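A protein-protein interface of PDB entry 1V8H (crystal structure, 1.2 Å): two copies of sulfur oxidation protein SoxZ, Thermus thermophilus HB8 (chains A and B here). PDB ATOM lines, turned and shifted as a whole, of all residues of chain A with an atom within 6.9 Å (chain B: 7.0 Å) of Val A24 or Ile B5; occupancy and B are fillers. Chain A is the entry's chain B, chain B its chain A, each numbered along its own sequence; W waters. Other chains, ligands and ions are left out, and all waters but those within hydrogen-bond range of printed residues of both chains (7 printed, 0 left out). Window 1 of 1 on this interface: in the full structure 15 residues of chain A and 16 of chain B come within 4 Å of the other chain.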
ATOM      1  N   PHE A   2      23.717  22.529  19.160  1.00  0.00           N
ATOM      2  CA  PHE A   2      23.514  22.532  17.715  1.00  0.00           C
ATOM      3  C   PHE A   2      24.836  22.531  16.941  1.00  0.00           C
ATOM      4  O   PHE A   2      25.842  23.104  17.344  1.00  0.00           O
ATOM      5  CB  PHE A   2      22.645  23.732  17.321  1.00  0.00           C
ATOM      6  CG  PHE A   2      23.191  25.001  17.910  1.00  0.00           C
ATOM      7  CD1 PHE A   2      24.090  25.764  17.175  1.00  0.00           C
ATOM      8  CD2 PHE A   2      22.717  25.465  19.128  1.00  0.00           C
ATOM      9  CE1 PHE A   2      24.513  26.994  17.660  1.00  0.00           C
ATOM     10  CE2 PHE A   2      23.145  26.702  19.608  1.00  0.00           C
ATOM     11  CZ  PHE A   2      24.046  27.468  18.878  1.00  0.00           C
ATOM     12  N   ARG A   3      24.814  21.812  15.806  1.00  0.00           N
ATOM     13  CA  ARG A   3      26.031  21.621  15.022  1.00  0.00           C
ATOM     14  C   ARG A   3      26.626  22.947  14.539  1.00  0.00           C
ATOM     15  O   ARG A   3      25.926  23.839  14.077  1.00  0.00           O
ATOM     16  CB  ARG A   3      25.667  20.748  13.824  1.00  0.00           C
ATOM     17  CG  ARG A   3      26.892  20.180  13.110  1.00  0.00           C
ATOM     18  CD  ARG A   3      26.500  19.125  12.071  1.00  0.00           C
ATOM     19  NE  ARG A   3      25.866  17.975  12.721  1.00  0.00           N
ATOM     20  CZ  ARG A   3      24.525  17.988  12.835  1.00  0.00           C
ATOM     21  NH1 ARG A   3      23.828  19.011  12.372  1.00  0.00           N
ATOM     22  NH2 ARG A   3      23.902  16.953  13.404  1.00  0.00           N
ATOM     23  N   THR A   4      27.950  23.013  14.649  1.00  0.00           N
ATOM     24  CA  THR A   4      28.702  24.189  14.246  1.00  0.00           C
ATOM     25  C   THR A   4      30.010  23.729  13.618  1.00  0.00           C
ATOM     26  O   THR A   4      30.621  22.765  14.084  1.00  0.00           O
ATOM     27  CB  THR A   4      29.036  25.064  15.473  1.00  0.00           C
ATOM     28  OG1 THR A   4      27.830  25.379  16.178  1.00  0.00           O
ATOM     29  CG2 THR A   4      29.726  26.349  15.050  1.00  0.00           C
ATOM     30  N   ILE A   5      30.435  24.408  12.559  1.00  0.00           N
ATOM     31  CA  ILE A   5      31.687  24.080  11.892  1.00  0.00           C
ATOM     32  C   ILE A   5      32.425  25.376  11.599  1.00  0.00           C
ATOM     33  O   ILE A   5      31.826  26.356  11.149  1.00  0.00           O
ATOM     34  CB  ILE A   5      31.454  23.331  10.552  1.00  0.00           C
ATOM     35  CG1 ILE A   5      30.774  21.985  10.814  1.00  0.00           C
ATOM     36  CG2 ILE A   5      32.789  23.107   9.837  1.00  0.00           C
ATOM     37  CD1 ILE A   5      30.338  21.253   9.554  1.00  0.00           C
ATOM     38  N   ALA A   6      33.726  25.379  11.868  1.00  0.00           N
ATOM     39  CA  ALA A   6      34.567  26.538  11.610  1.00  0.00           C
ATOM     40  C   ALA A   6      35.576  26.168  10.527  1.00  0.00           C
ATOM     41  O   ALA A   6      36.062  25.030  10.477  1.00  0.00           O
ATOM     42  CB  ALA A   6      35.297  26.954  12.883  1.00  0.00           C
ATOM     43  N   ARG A   7      35.880  27.120   9.655  1.00  0.00           N
ATOM     44  CA  ARG A   7      36.847  26.884   8.597  1.00  0.00           C
ATOM     45  C   ARG A   7      37.646  28.150   8.345  1.00  0.00           C
ATOM     46  O   ARG A   7      37.216  29.258   8.689  1.00  0.00           O
ATOM     47  CB  ARG A   7      36.149  26.429   7.311  1.00  0.00           C
ATOM     48  CG  ARG A   7      35.235  27.462   6.679  1.00  0.00           C
ATOM     49  CD  ARG A   7      34.421  26.862   5.535  1.00  0.00           C
ATOM     50  NE  ARG A   7      35.257  26.414   4.423  1.00  0.00           N
ATOM     51  CZ  ARG A   7      35.584  27.166   3.376  1.00  0.00           C
ATOM     52  NH1 ARG A   7      35.146  28.413   3.286  1.00  0.00           N
ATOM     53  NH2 ARG A   7      36.348  26.671   2.412  1.00  0.00           N
ATOM     54  N   GLN A  22      35.409  31.445   9.000  1.00  0.00           N
ATOM     55  CA  GLN A  22      33.979  31.367   8.772  1.00  0.00           C
ATOM     56  C   GLN A  22      33.421  30.376   9.766  1.00  0.00           C
ATOM     57  O   GLN A  22      34.012  29.319  10.010  1.00  0.00           O
ATOM     58  CB  GLN A  22      33.655  30.878   7.365  1.00  0.00           C
ATOM     59  CG  GLN A  22      34.025  31.835   6.259  1.00  0.00           C
ATOM     60  CD  GLN A  22      33.603  31.307   4.910  1.00  0.00           C
ATOM     61  OE1 GLN A  22      33.849  30.146   4.591  1.00  0.00           O
ATOM     62  NE2 GLN A  22      32.965  32.151   4.106  1.00  0.00           N
ATOM     63  N   VAL A  23      32.280  30.728  10.340  1.00  0.00           N
ATOM     64  CA  VAL A  23      31.605  29.874  11.297  1.00  0.00           C
ATOM     65  C   VAL A  23      30.193  29.664  10.773  1.00  0.00           C
ATOM     66  O   VAL A  23      29.473  30.632  10.511  1.00  0.00           O
ATOM     67  CB  VAL A  23      31.517  30.547  12.682  1.00  0.00           C
ATOM     68  CG1 VAL A  23      30.788  29.634  13.658  1.00  0.00           C
ATOM     69  CG2 VAL A  23      32.909  30.892  13.187  1.00  0.00           C
ATOM     70  N   VAL A  24      29.808  28.405  10.597  1.00  0.00           N
ATOM     71  CA  VAL A  24      28.470  28.086  10.132  1.00  0.00           C
ATOM     72  C   VAL A  24      27.787  27.241  11.193  1.00  0.00           C
ATOM     73  O   VAL A  24      28.404  26.371  11.813  1.00  0.00           O
ATOM     74  CB  VAL A  24      28.493  27.305   8.803  1.00  0.00           C
ATOM     75  CG1 VAL A  24      27.083  26.888   8.421  1.00  0.00           C
ATOM     76  CG2 VAL A  24      29.102  28.163   7.710  1.00  0.00           C
ATOM     77  N   ALA A  25      26.509  27.512  11.416  1.00  0.00           N
ATOM     78  CA  ALA A  25      25.754  26.762  12.403  1.00  0.00           C
ATOM     79  C   ALA A  25      24.469  26.234  11.796  1.00  0.00           C
ATOM     80  O   ALA A  25      23.900  26.849  10.886  1.00  0.00           O
ATOM     81  CB  ALA A  25      25.425  27.653  13.590  1.00  0.00           C
ATOM     82  N   GLN A  26      24.033  25.073  12.274  1.00  0.00           N
ATOM     83  CA  GLN A  26      22.768  24.512  11.832  1.00  0.00           C
ATOM     84  C   GLN A  26      21.817  25.034  12.904  1.00  0.00           C
ATOM     85  O   GLN A  26      21.894  24.625  14.066  1.00  0.00           O
ATOM     86  CB  GLN A  26      22.788  22.986  11.854  1.00  0.00           C
ATOM     87  CG  GLN A  26      21.479  22.374  11.369  1.00  0.00           C
ATOM     88  CD  GLN A  26      21.473  20.863  11.455  1.00  0.00           C
ATOM     89  OE1 GLN A  26      21.478  20.294  12.545  1.00  0.00           O
ATOM     90  NE2 GLN A  26      21.467  20.204  10.302  1.00  0.00           N
ATOM     91  N   HIS A  27      20.939  25.951  12.523  1.00  0.00           N
ATOM     92  CA  HIS A  27      20.023  26.543  13.482  1.00  0.00           C
ATOM     93  C   HIS A  27      18.882  27.214  12.736  1.00  0.00           C
ATOM     94  O   HIS A  27      19.105  27.918  11.755  1.00  0.00           O
ATOM     95  CB  HIS A  27      20.775  27.575  14.323  1.00  0.00           C
ATOM     96  CG  HIS A  27      20.098  27.908  15.613  1.00  0.00           C
ATOM     97  ND1 HIS A  27      18.941  28.654  15.682  1.00  0.00           N
ATOM     98  CD2 HIS A  27      20.394  27.552  16.884  1.00  0.00           C
ATOM     99  CE1 HIS A  27      18.552  28.742  16.942  1.00  0.00           C
ATOM    100  NE2 HIS A  27      19.417  28.081  17.693  1.00  0.00           N
ATOM    101  N   ASN A  71      20.432  28.663   9.509  1.00  0.00           N
ATOM    102  CA  ASN A  71      21.774  28.121   9.272  1.00  0.00           C
ATOM    103  C   ASN A  71      22.713  29.237   8.871  1.00  0.00           C
ATOM    104  O   ASN A  71      23.266  29.261   7.768  1.00  0.00           O
ATOM    105  CB  ASN A  71      21.683  27.043   8.204  1.00  0.00           C
ATOM    106  CG  ASN A  71      20.551  26.093   8.487  1.00  0.00           C
ATOM    107  OD1 ASN A  71      20.453  25.559   9.594  1.00  0.00           O
ATOM    108  ND2 ASN A  71      19.665  25.904   7.511  1.00  0.00           N
ATOM    109  N   PRO A  72      22.941  30.166   9.801  1.00  0.00           N
ATOM    110  CA  PRO A  72      23.797  31.323   9.579  1.00  0.00           C
ATOM    111  C   PRO A  72      25.280  31.092   9.399  1.00  0.00           C
ATOM    112  O   PRO A  72      25.849  30.101   9.859  1.00  0.00           O
ATOM    113  CB  PRO A  72      23.510  32.185  10.796  1.00  0.00           C
ATOM    114  CG  PRO A  72      23.371  31.158  11.865  1.00  0.00           C
ATOM    115  CD  PRO A  72      22.488  30.121  11.205  1.00  0.00           C
ATOM    116  N   LEU A  73      25.890  32.061   8.728  1.00  0.00           N
ATOM    117  CA  LEU A  73      27.319  32.093   8.477  1.00  0.00           C
ATOM    118  C   LEU A  73      27.828  33.417   9.043  1.00  0.00           C
ATOM    119  O   LEU A  73      27.262  34.480   8.771  1.00  0.00           O
ATOM    120  CB  LEU A  73      27.602  32.024   6.974  1.00  0.00           C
ATOM    121  CG  LEU A  73      28.964  32.570   6.529  1.00  0.00           C
ATOM    122  CD1 LEU A  73      30.078  31.699   7.081  1.00  0.00           C
ATOM    123  CD2 LEU A  73      29.025  32.618   5.013  1.00  0.00           C
ATOM    124  N   TYR A  74      28.874  33.348   9.857  1.00  0.00           N
ATOM    125  CA  TYR A  74      29.496  34.534  10.437  1.00  0.00           C
ATOM    126  C   TYR A  74      30.947  34.462   9.977  1.00  0.00           C
ATOM    127  O   TYR A  74      31.577  33.406  10.078  1.00  0.00           O
ATOM    128  CB  TYR A  74      29.463  34.487  11.965  1.00  0.00           C
ATOM    129  CG  TYR A  74      28.115  34.168  12.558  1.00  0.00           C
ATOM    130  CD1 TYR A  74      27.103  35.125  12.617  1.00  0.00           C
ATOM    131  CD2 TYR A  74      27.852  32.898  13.068  1.00  0.00           C
ATOM    132  CE1 TYR A  74      25.858  34.821  13.172  1.00  0.00           C
ATOM    133  CE2 TYR A  74      26.622  32.583  13.618  1.00  0.00           C
ATOM    134  CZ  TYR A  74      25.630  33.543  13.671  1.00  0.00           C
ATOM    135  OH  TYR A  74      24.423  33.203  14.234  1.00  0.00           O
ATOM    136  N   LEU A  90      28.933  29.402  20.527  1.00  0.00           N
ATOM    137  CA  LEU A  90      27.667  30.044  20.204  1.00  0.00           C
ATOM    138  C   LEU A  90      26.610  29.713  21.257  1.00  0.00           C
ATOM    139  O   LEU A  90      26.629  28.669  21.897  1.00  0.00           O
ATOM    140  CB  LEU A  90      27.194  29.498  18.856  1.00  0.00           C
ATOM    141  CG  LEU A  90      28.168  29.772  17.707  1.00  0.00           C
ATOM    142  CD1 LEU A  90      29.413  28.879  17.756  1.00  0.00           C
ATOM    143  CD2 LEU A  90      27.523  29.533  16.345  1.00  0.00           C
ATOM    144  N   ALA A 100      32.853  25.018  18.164  1.00  0.00           N
ATOM    145  CA  ALA A 100      33.714  24.456  17.141  1.00  0.00           C
ATOM    146  C   ALA A 100      35.133  24.980  17.290  1.00  0.00           C
ATOM    147  O   ALA A 100      35.397  25.992  17.933  1.00  0.00           O
ATOM    148  CB  ALA A 100      33.155  24.842  15.772  1.00  0.00           C
ATOM    149  N   PHE B   2      31.674  12.348   9.460  1.00  0.00           N
ATOM    150  CA  PHE B   2      32.212  13.674   9.730  1.00  0.00           C
ATOM    151  C   PHE B   2      31.106  14.723   9.664  1.00  0.00           C
ATOM    152  O   PHE B   2      30.166  14.603   8.873  1.00  0.00           O
ATOM    153  CB  PHE B   2      33.367  14.005   8.768  1.00  0.00           C
ATOM    154  CG  PHE B   2      33.086  13.708   7.316  1.00  0.00           C
ATOM    155  CD1 PHE B   2      32.470  14.652   6.500  1.00  0.00           C
ATOM    156  CD2 PHE B   2      33.484  12.495   6.751  1.00  0.00           C
ATOM    157  CE1 PHE B   2      32.260  14.396   5.148  1.00  0.00           C
ATOM    158  CE2 PHE B   2      33.277  12.231   5.401  1.00  0.00           C
ATOM    159  CZ  PHE B   2      32.665  13.184   4.598  1.00  0.00           C
ATOM    160  N   ARG B   3      31.216  15.741  10.512  1.00  0.00           N
ATOM    161  CA  ARG B   3      30.217  16.802  10.576  1.00  0.00           C
ATOM    162  C   ARG B   3      30.022  17.527   9.258  1.00  0.00           C
ATOM    163  O   ARG B   3      30.985  17.866   8.573  1.00  0.00           O
ATOM    164  CB  ARG B   3      30.591  17.825  11.653  1.00  0.00           C
ATOM    165  CG  ARG B   3      30.598  17.291  13.072  1.00  0.00           C
ATOM    166  CD  ARG B   3      30.652  18.433  14.079  1.00  0.00           C
ATOM    167  NE  ARG B   3      30.684  17.949  15.454  1.00  0.00           N
ATOM    168  CZ  ARG B   3      31.776  17.511  16.070  1.00  0.00           C
ATOM    169  NH1 ARG B   3      32.940  17.496  15.435  1.00  0.00           N
ATOM    170  NH2 ARG B   3      31.705  17.085  17.325  1.00  0.00           N
ATOM    171  N   THR B   4      28.759  17.772   8.919  1.00  0.00           N
ATOM    172  CA  THR B   4      28.398  18.478   7.699  1.00  0.00           C
ATOM    173  C   THR B   4      27.175  19.348   7.986  1.00  0.00           C
ATOM    174  O   THR B   4      26.292  18.958   8.756  1.00  0.00           O
ATOM    175  CB  THR B   4      28.031  17.495   6.558  1.00  0.00           C
ATOM    176  OG1 THR B   4      29.130  16.609   6.314  1.00  0.00           O
ATOM    177  CG2 THR B   4      27.717  18.245   5.279  1.00  0.00           C
ATOM    178  N   ILE B   5      27.146  20.533   7.385  1.00  0.00           N
ATOM    179  CA  ILE B   5      26.018  21.447   7.536  1.00  0.00           C
ATOM    180  C   ILE B   5      25.646  21.956   6.156  1.00  0.00           C
ATOM    181  O   ILE B   5      26.512  22.314   5.359  1.00  0.00           O
ATOM    182  CB  ILE B   5      26.364  22.675   8.408  1.00  0.00           C
ATOM    183  CG1 ILE B   5      26.677  22.233   9.838  1.00  0.00           C
ATOM    184  CG2 ILE B   5      25.194  23.669   8.399  1.00  0.00           C
ATOM    185  CD1 ILE B   5      27.177  23.363  10.732  1.00  0.00           C
ATOM    186  N   ALA B   6      24.349  21.981   5.880  1.00  0.00           N
ATOM    187  CA  ALA B   6      23.838  22.465   4.608  1.00  0.00           C
ATOM    188  C   ALA B   6      23.047  23.744   4.856  1.00  0.00           C
ATOM    189  O   ALA B   6      22.295  23.839   5.828  1.00  0.00           O
ATOM    190  CB  ALA B   6      22.940  21.418   3.976  1.00  0.00           C
ATOM    191  N   ARG B   7      23.225  24.729   3.987  1.00  0.00           N
ATOM    192  CA  ARG B   7      22.490  25.979   4.124  1.00  0.00           C
ATOM    193  C   ARG B   7      22.097  26.497   2.746  1.00  0.00           C
ATOM    194  O   ARG B   7      22.698  26.131   1.730  1.00  0.00           O
ATOM    195  CB  ARG B   7      23.330  27.026   4.874  1.00  0.00           C
ATOM    196  CG  ARG B   7      24.564  27.521   4.134  1.00  0.00           C
ATOM    197  CD  ARG B   7      25.447  28.381   5.044  1.00  0.00           C
ATOM    198  NE  ARG B   7      24.813  29.634   5.449  1.00  0.00           N
ATOM    199  CZ  ARG B   7      25.038  30.815   4.878  1.00  0.00           C
ATOM    200  NH1 ARG B   7      25.890  30.918   3.867  1.00  0.00           N
ATOM    201  NH2 ARG B   7      24.418  31.900   5.321  1.00  0.00           N
ATOM    202  N   GLN B  22      24.788  25.529  -0.113  1.00  0.00           N
ATOM    203  CA  GLN B  22      26.167  25.463   0.349  1.00  0.00           C
ATOM    204  C   GLN B  22      26.288  24.342   1.359  1.00  0.00           C
ATOM    205  O   GLN B  22      25.476  24.223   2.283  1.00  0.00           O
ATOM    206  CB  GLN B  22      26.583  26.763   1.025  1.00  0.00           C
ATOM    207  CG  GLN B  22      26.585  27.972   0.129  1.00  0.00           C
ATOM    208  CD  GLN B  22      26.924  29.228   0.895  1.00  0.00           C
ATOM    209  OE1 GLN B  22      26.292  29.535   1.902  1.00  0.00           O
ATOM    210  NE2 GLN B  22      27.924  29.962   0.424  1.00  0.00           N
ATOM    211  N   VAL B  23      27.312  23.518   1.185  1.00  0.00           N
ATOM    212  CA  VAL B  23      27.548  22.408   2.089  1.00  0.00           C
ATOM    213  C   VAL B  23      28.952  22.531   2.655  1.00  0.00           C
ATOM    214  O   VAL B  23      29.923  22.574   1.901  1.00  0.00           O
ATOM    215  CB  VAL B  23      27.414  21.064   1.354  1.00  0.00           C
ATOM    216  CG1 VAL B  23      27.634  19.913   2.328  1.00  0.00           C
ATOM    217  CG2 VAL B  23      26.039  20.970   0.703  1.00  0.00           C
ATOM    218  N   VAL B  24      29.058  22.616   3.975  1.00  0.00           N
ATOM    219  CA  VAL B  24      30.351  22.690   4.599  1.00  0.00           C
ATOM    220  C   VAL B  24      30.599  21.415   5.368  1.00  0.00           C
ATOM    221  O   VAL B  24      29.731  20.881   6.047  1.00  0.00           O
ATOM    222  CB  VAL B  24      30.376  23.872   5.559  1.00  0.00           C
ATOM    223  CG1 VAL B  24      31.822  23.890   6.273  1.00  0.00           C
ATOM    224  CG2 VAL B  24      30.246  25.186   4.845  1.00  0.00           C
ATOM    225  N   ALA B  25      31.806  20.884   5.228  1.00  0.00           N
ATOM    226  CA  ALA B  25      32.163  19.654   5.905  1.00  0.00           C
ATOM    227  C   ALA B  25      33.373  19.889   6.791  1.00  0.00           C
ATOM    228  O   ALA B  25      34.270  20.655   6.442  1.00  0.00           O
ATOM    229  CB  ALA B  25      32.482  18.565   4.885  1.00  0.00           C
ATOM    230  N   GLN B  26      33.377  19.262   7.957  1.00  0.00           N
ATOM    231  CA  GLN B  26      34.519  19.348   8.851  1.00  0.00           C
ATOM    232  C   GLN B  26      35.331  18.139   8.402  1.00  0.00           C
ATOM    233  O   GLN B  26      34.941  16.997   8.657  1.00  0.00           O
ATOM    234  CB  GLN B  26      34.065  19.187  10.291  1.00  0.00           C
ATOM    235  CG  GLN B  26      35.141  19.437  11.313  1.00  0.00           C
ATOM    236  CD  GLN B  26      34.574  19.429  12.710  1.00  0.00           C
ATOM    237  OE1 GLN B  26      34.292  18.368  13.265  1.00  0.00           O
ATOM    238  NE2 GLN B  26      34.384  20.613  13.282  1.00  0.00           N
ATOM    239  N   LEU B  73      34.017  23.777   1.480  1.00  0.00           N
ATOM    240  CA  LEU B  73      32.685  24.300   1.235  1.00  0.00           C
ATOM    241  C   LEU B  73      32.371  23.950  -0.218  1.00  0.00           C
ATOM    242  O   LEU B  73      33.188  24.189  -1.108  1.00  0.00           O
ATOM    243  CB  LEU B  73      32.658  25.825   1.436  1.00  0.00           C
ATOM    244  CG  LEU B  73      31.335  26.587   1.262  1.00  0.00           C
ATOM    245  CD1 LEU B  73      30.980  26.705  -0.207  1.00  0.00           C
ATOM    246  CD2 LEU B  73      30.232  25.889   2.024  1.00  0.00           C
ATOM    247  N   ILE B  88      22.248  15.851   1.205  1.00  0.00           N
ATOM    248  CA  ILE B  88      23.556  15.750   0.586  1.00  0.00           C
ATOM    249  C   ILE B  88      24.349  14.647   1.268  1.00  0.00           C
ATOM    250  O   ILE B  88      24.443  14.602   2.497  1.00  0.00           O
ATOM    251  CB  ILE B  88      24.329  17.084   0.691  1.00  0.00           C
ATOM    252  CG1 ILE B  88      23.482  18.237   0.133  1.00  0.00           C
ATOM    253  CG2 ILE B  88      25.633  16.984  -0.083  1.00  0.00           C
ATOM    254  CD1 ILE B  88      22.540  18.866   1.149  1.00  0.00           C
ATOM    255  N   GLU B  99      26.651  13.557   5.976  1.00  0.00           N
ATOM    256  CA  GLU B  99      25.312  13.754   5.441  1.00  0.00           C
ATOM    257  C   GLU B  99      24.655  14.951   6.099  1.00  0.00           C
ATOM    258  O   GLU B  99      24.804  15.168   7.300  1.00  0.00           O
ATOM    259  CB  GLU B  99      24.442  12.511   5.655  1.00  0.00           C
ATOM    260  CG  GLU B  99      23.073  12.633   4.995  1.00  0.00           C
ATOM    261  CD  GLU B  99      22.238  11.372   5.090  1.00  0.00           C
ATOM    262  OE1 GLU B  99      22.751  10.286   4.739  1.00  0.00           O
ATOM    263  OE2 GLU B  99      21.061  11.472   5.500  1.00  0.00           O
ATOM    264  N   ALA B 100      23.939  15.732   5.301  1.00  0.00           N
ATOM    265  CA  ALA B 100      23.235  16.895   5.817  1.00  0.00           C
ATOM    266  C   ALA B 100      21.984  17.114   4.987  1.00  0.00           C
ATOM    267  O   ALA B 100      21.871  16.611   3.872  1.00  0.00           O
ATOM    268  CB  ALA B 100      24.127  18.124   5.751  1.00  0.00           C
ATOM    269  N   SER B 101      21.036  17.856   5.543  1.00  0.00           N
ATOM    270  CA  SER B 101      19.802  18.166   4.835  1.00  0.00           C
ATOM    271  C   SER B 101      19.385  19.587   5.159  1.00  0.00           C
ATOM    272  O   SER B 101      19.773  20.137   6.186  1.00  0.00           O
ATOM    273  CB  SER B 101      18.674  17.217   5.251  1.00  0.00           C
ATOM    274  OG  SER B 101      18.948  15.879   4.881  1.00  0.00           O
ATOM    275  N   VAL B 102      18.617  20.185   4.259  1.00  0.00           N
ATOM    276  CA  VAL B 102      18.099  21.526   4.476  1.00  0.00           C
ATOM    277  C   VAL B 102      16.828  21.649   3.653  1.00  0.00           C
ATOM    278  O   VAL B 102      16.762  21.184   2.515  1.00  0.00           O
ATOM    279  CB  VAL B 102      19.120  22.633   4.086  1.00  0.00           C
ATOM    280  CG1 VAL B 102      19.433  22.581   2.601  1.00  0.00           C
ATOM    281  CG2 VAL B 102      18.571  24.001   4.472  1.00  0.00           C
HETATM  282  O   HOH W   1      22.584  20.952   7.853  1.00  0.00           O
HETATM  283  O   HOH W   2      26.560  16.155  10.311  1.00  0.00           O
HETATM  284  O   HOH W   3      29.165  20.855  16.343  1.00  0.00           O
HETATM  285  O   HOH W   4      21.905  31.846   6.442  1.00  0.00           O
HETATM  286  O   HOH W   5      32.147  20.980  15.604  1.00  0.00           O
HETATM  287  O   HOH W   6      21.287  17.918   8.567  1.00  0.00           O
HETATM  288  O   HOH W   7      35.459  23.202  12.591  1.00  0.00           O
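NE of Arg B7 sits at hydrogen-bond distance from O of Asn A71.
O of Phe B2 is in hydrogen-bond range of OG1 of Thr B4 (3.4 Å). NH1 of Arg B3 is in hydrogen-bond range of OE1 of Gln B26, 2.7 Å away. The backbone carbonyl oxygen (O) of Ile B5 is in hydrogen-bond range of the backbone NH (N) of Val B24. The guanidinium group of Arg A3 lies within hydrogen-bond range of the side-chain amide oxygen of Gln A26. The backbone NH (N) of Ile A5 lies within hydrogen-bond range of the backbone carbonyl oxygen (O) of Val A24 (2.9 Å). The backbone carbonyl oxygen of His A27 is in hydrogen-bond range of the backbone NH of Asn A71, at 2.7 Å.
Among the printed residues, pairs that only touch across the chains: Arg A3 with Thr B4 (3.3 Å), Arg A3 with Ile B5 (3.6 Å), Thr A4 with Ile B5 (3.9 Å), Ile A5 with Arg B3 (3.6 Å), Ile A5 with Thr B4 (3.9 Å), Ile A5 with Ile B5 (3.8 Å), Ile A5 with Val B24 (3.6 Å), Ile A5 with Gln B26 (3.97 Å), Arg A7 with Leu B73 (3.8 Å), Val A24 with Ile B5 (3.4 Å), Gln A26 with Ile B5 (3.9 Å), Asn A71 with Ala B6 (3.7 Å), Asn A71 with Val B102 (3.7 Å) and Leu A73 with Arg B7 (3.5 Å).
Printed residues of chain B within 4 Å of Thr A4: Ile B5. Of the printed residues of chain B, Arg A7 touches Leu B73 (3.8 Å). Val A24 touches just one residue of chain B: Ile B5 (3.4 Å). Printed residues of chain B within 4 Å of Asn A71: Ala B6, Arg B7 and Val B102. Leu A90 touches none of the printed residues of chain B. Printed residues of chain A within 4 Å of Ile B5: Arg A3 (3.6 Å), Thr A4 (3.9 Å), Ile A5 (3.8 Å), Val A24 (3.4 Å) and Gln A26 (3.9 Å). Ala B25 touches none of the printed residues of chain A. Printed residues of chain A within 4 Å of Gln B26: Ile A5 (3.97 Å). Printed residues of chain A within 4 Å of Val B102: Asn A71 (3.7 Å). The nearest residue of chain B that does not touch Val A24 is Arg B7 (4.04 Å). The nearest printed residue of chain A that does not touch Ile B5 is Ala A25 (4.05 Å). The nearest printed residue of chain B that does not touch Arg A3 is Arg B3 (4.3 Å).
Of the 17 printed residues of chain B, 9 touch a printed residue of chain A. Printed residues of chain B that touch a printed residue of chain A: Arg B3, Thr B4, Ile B5, Ala B6, Arg B7, Val B24, Gln B26, Leu B73 and Val B102. Hydrophobic or aromatic side chains of chain B within 4 Å of the printed part of chain A: Ile B5, Val B24, Leu B73 and Val B102.
Arg A3 touches Thr B4, but with the chains exchanged Thr A4 does not touch Arg B3 (4.3 Å). Thr A4 touches Ile B5, and with the chains exchanged Ile A5 touches Thr B4. Ile A5 touches Gln B26, and with the chains exchanged Gln A26 touches Ile B5. Arg A7 touches Leu B73, and with the chains exchanged Leu A73 touches Arg B7. 13 positions are printed for both chains. Of the 15 pairs that touch across the chains among the printed residues, 11 have their exchanged pair printed and touching as well.
Water W4 lies within hydrogen-bond range of NH2 of Arg B7 (2.8 Å) and O of Asn A71 (3.2 Å). Water W1 lies within hydrogen-bond range of NE2 of Gln A26 (2.8 Å), N of Ala B6 (2.8 Å) and O of Ser B101 (3.4 Å). Water W5 lies within hydrogen-bond range of the backbone carbonyl oxygen of Thr A4 (2.8 Å), the side-chain amide nitrogen of Gln B26 (3.2 Å) and the guanidinium group of Arg B3 (3.4 Å). Water W7 lies within hydrogen-bond range of the backbone carbonyl oxygen (O) of Ala A6 and the side-chain amide nitrogen (NE2) of Gln B26. Water W3 bridges the backbone NH (N) of Thr A4 (3.0 Å) and the guanidinium group (NE) of Arg B3 (3.4 Å). Water W2 bridges the backbone NH of Thr B4 (3.1 Å) and the guanidinium group of Arg A3 (3.1 Å).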
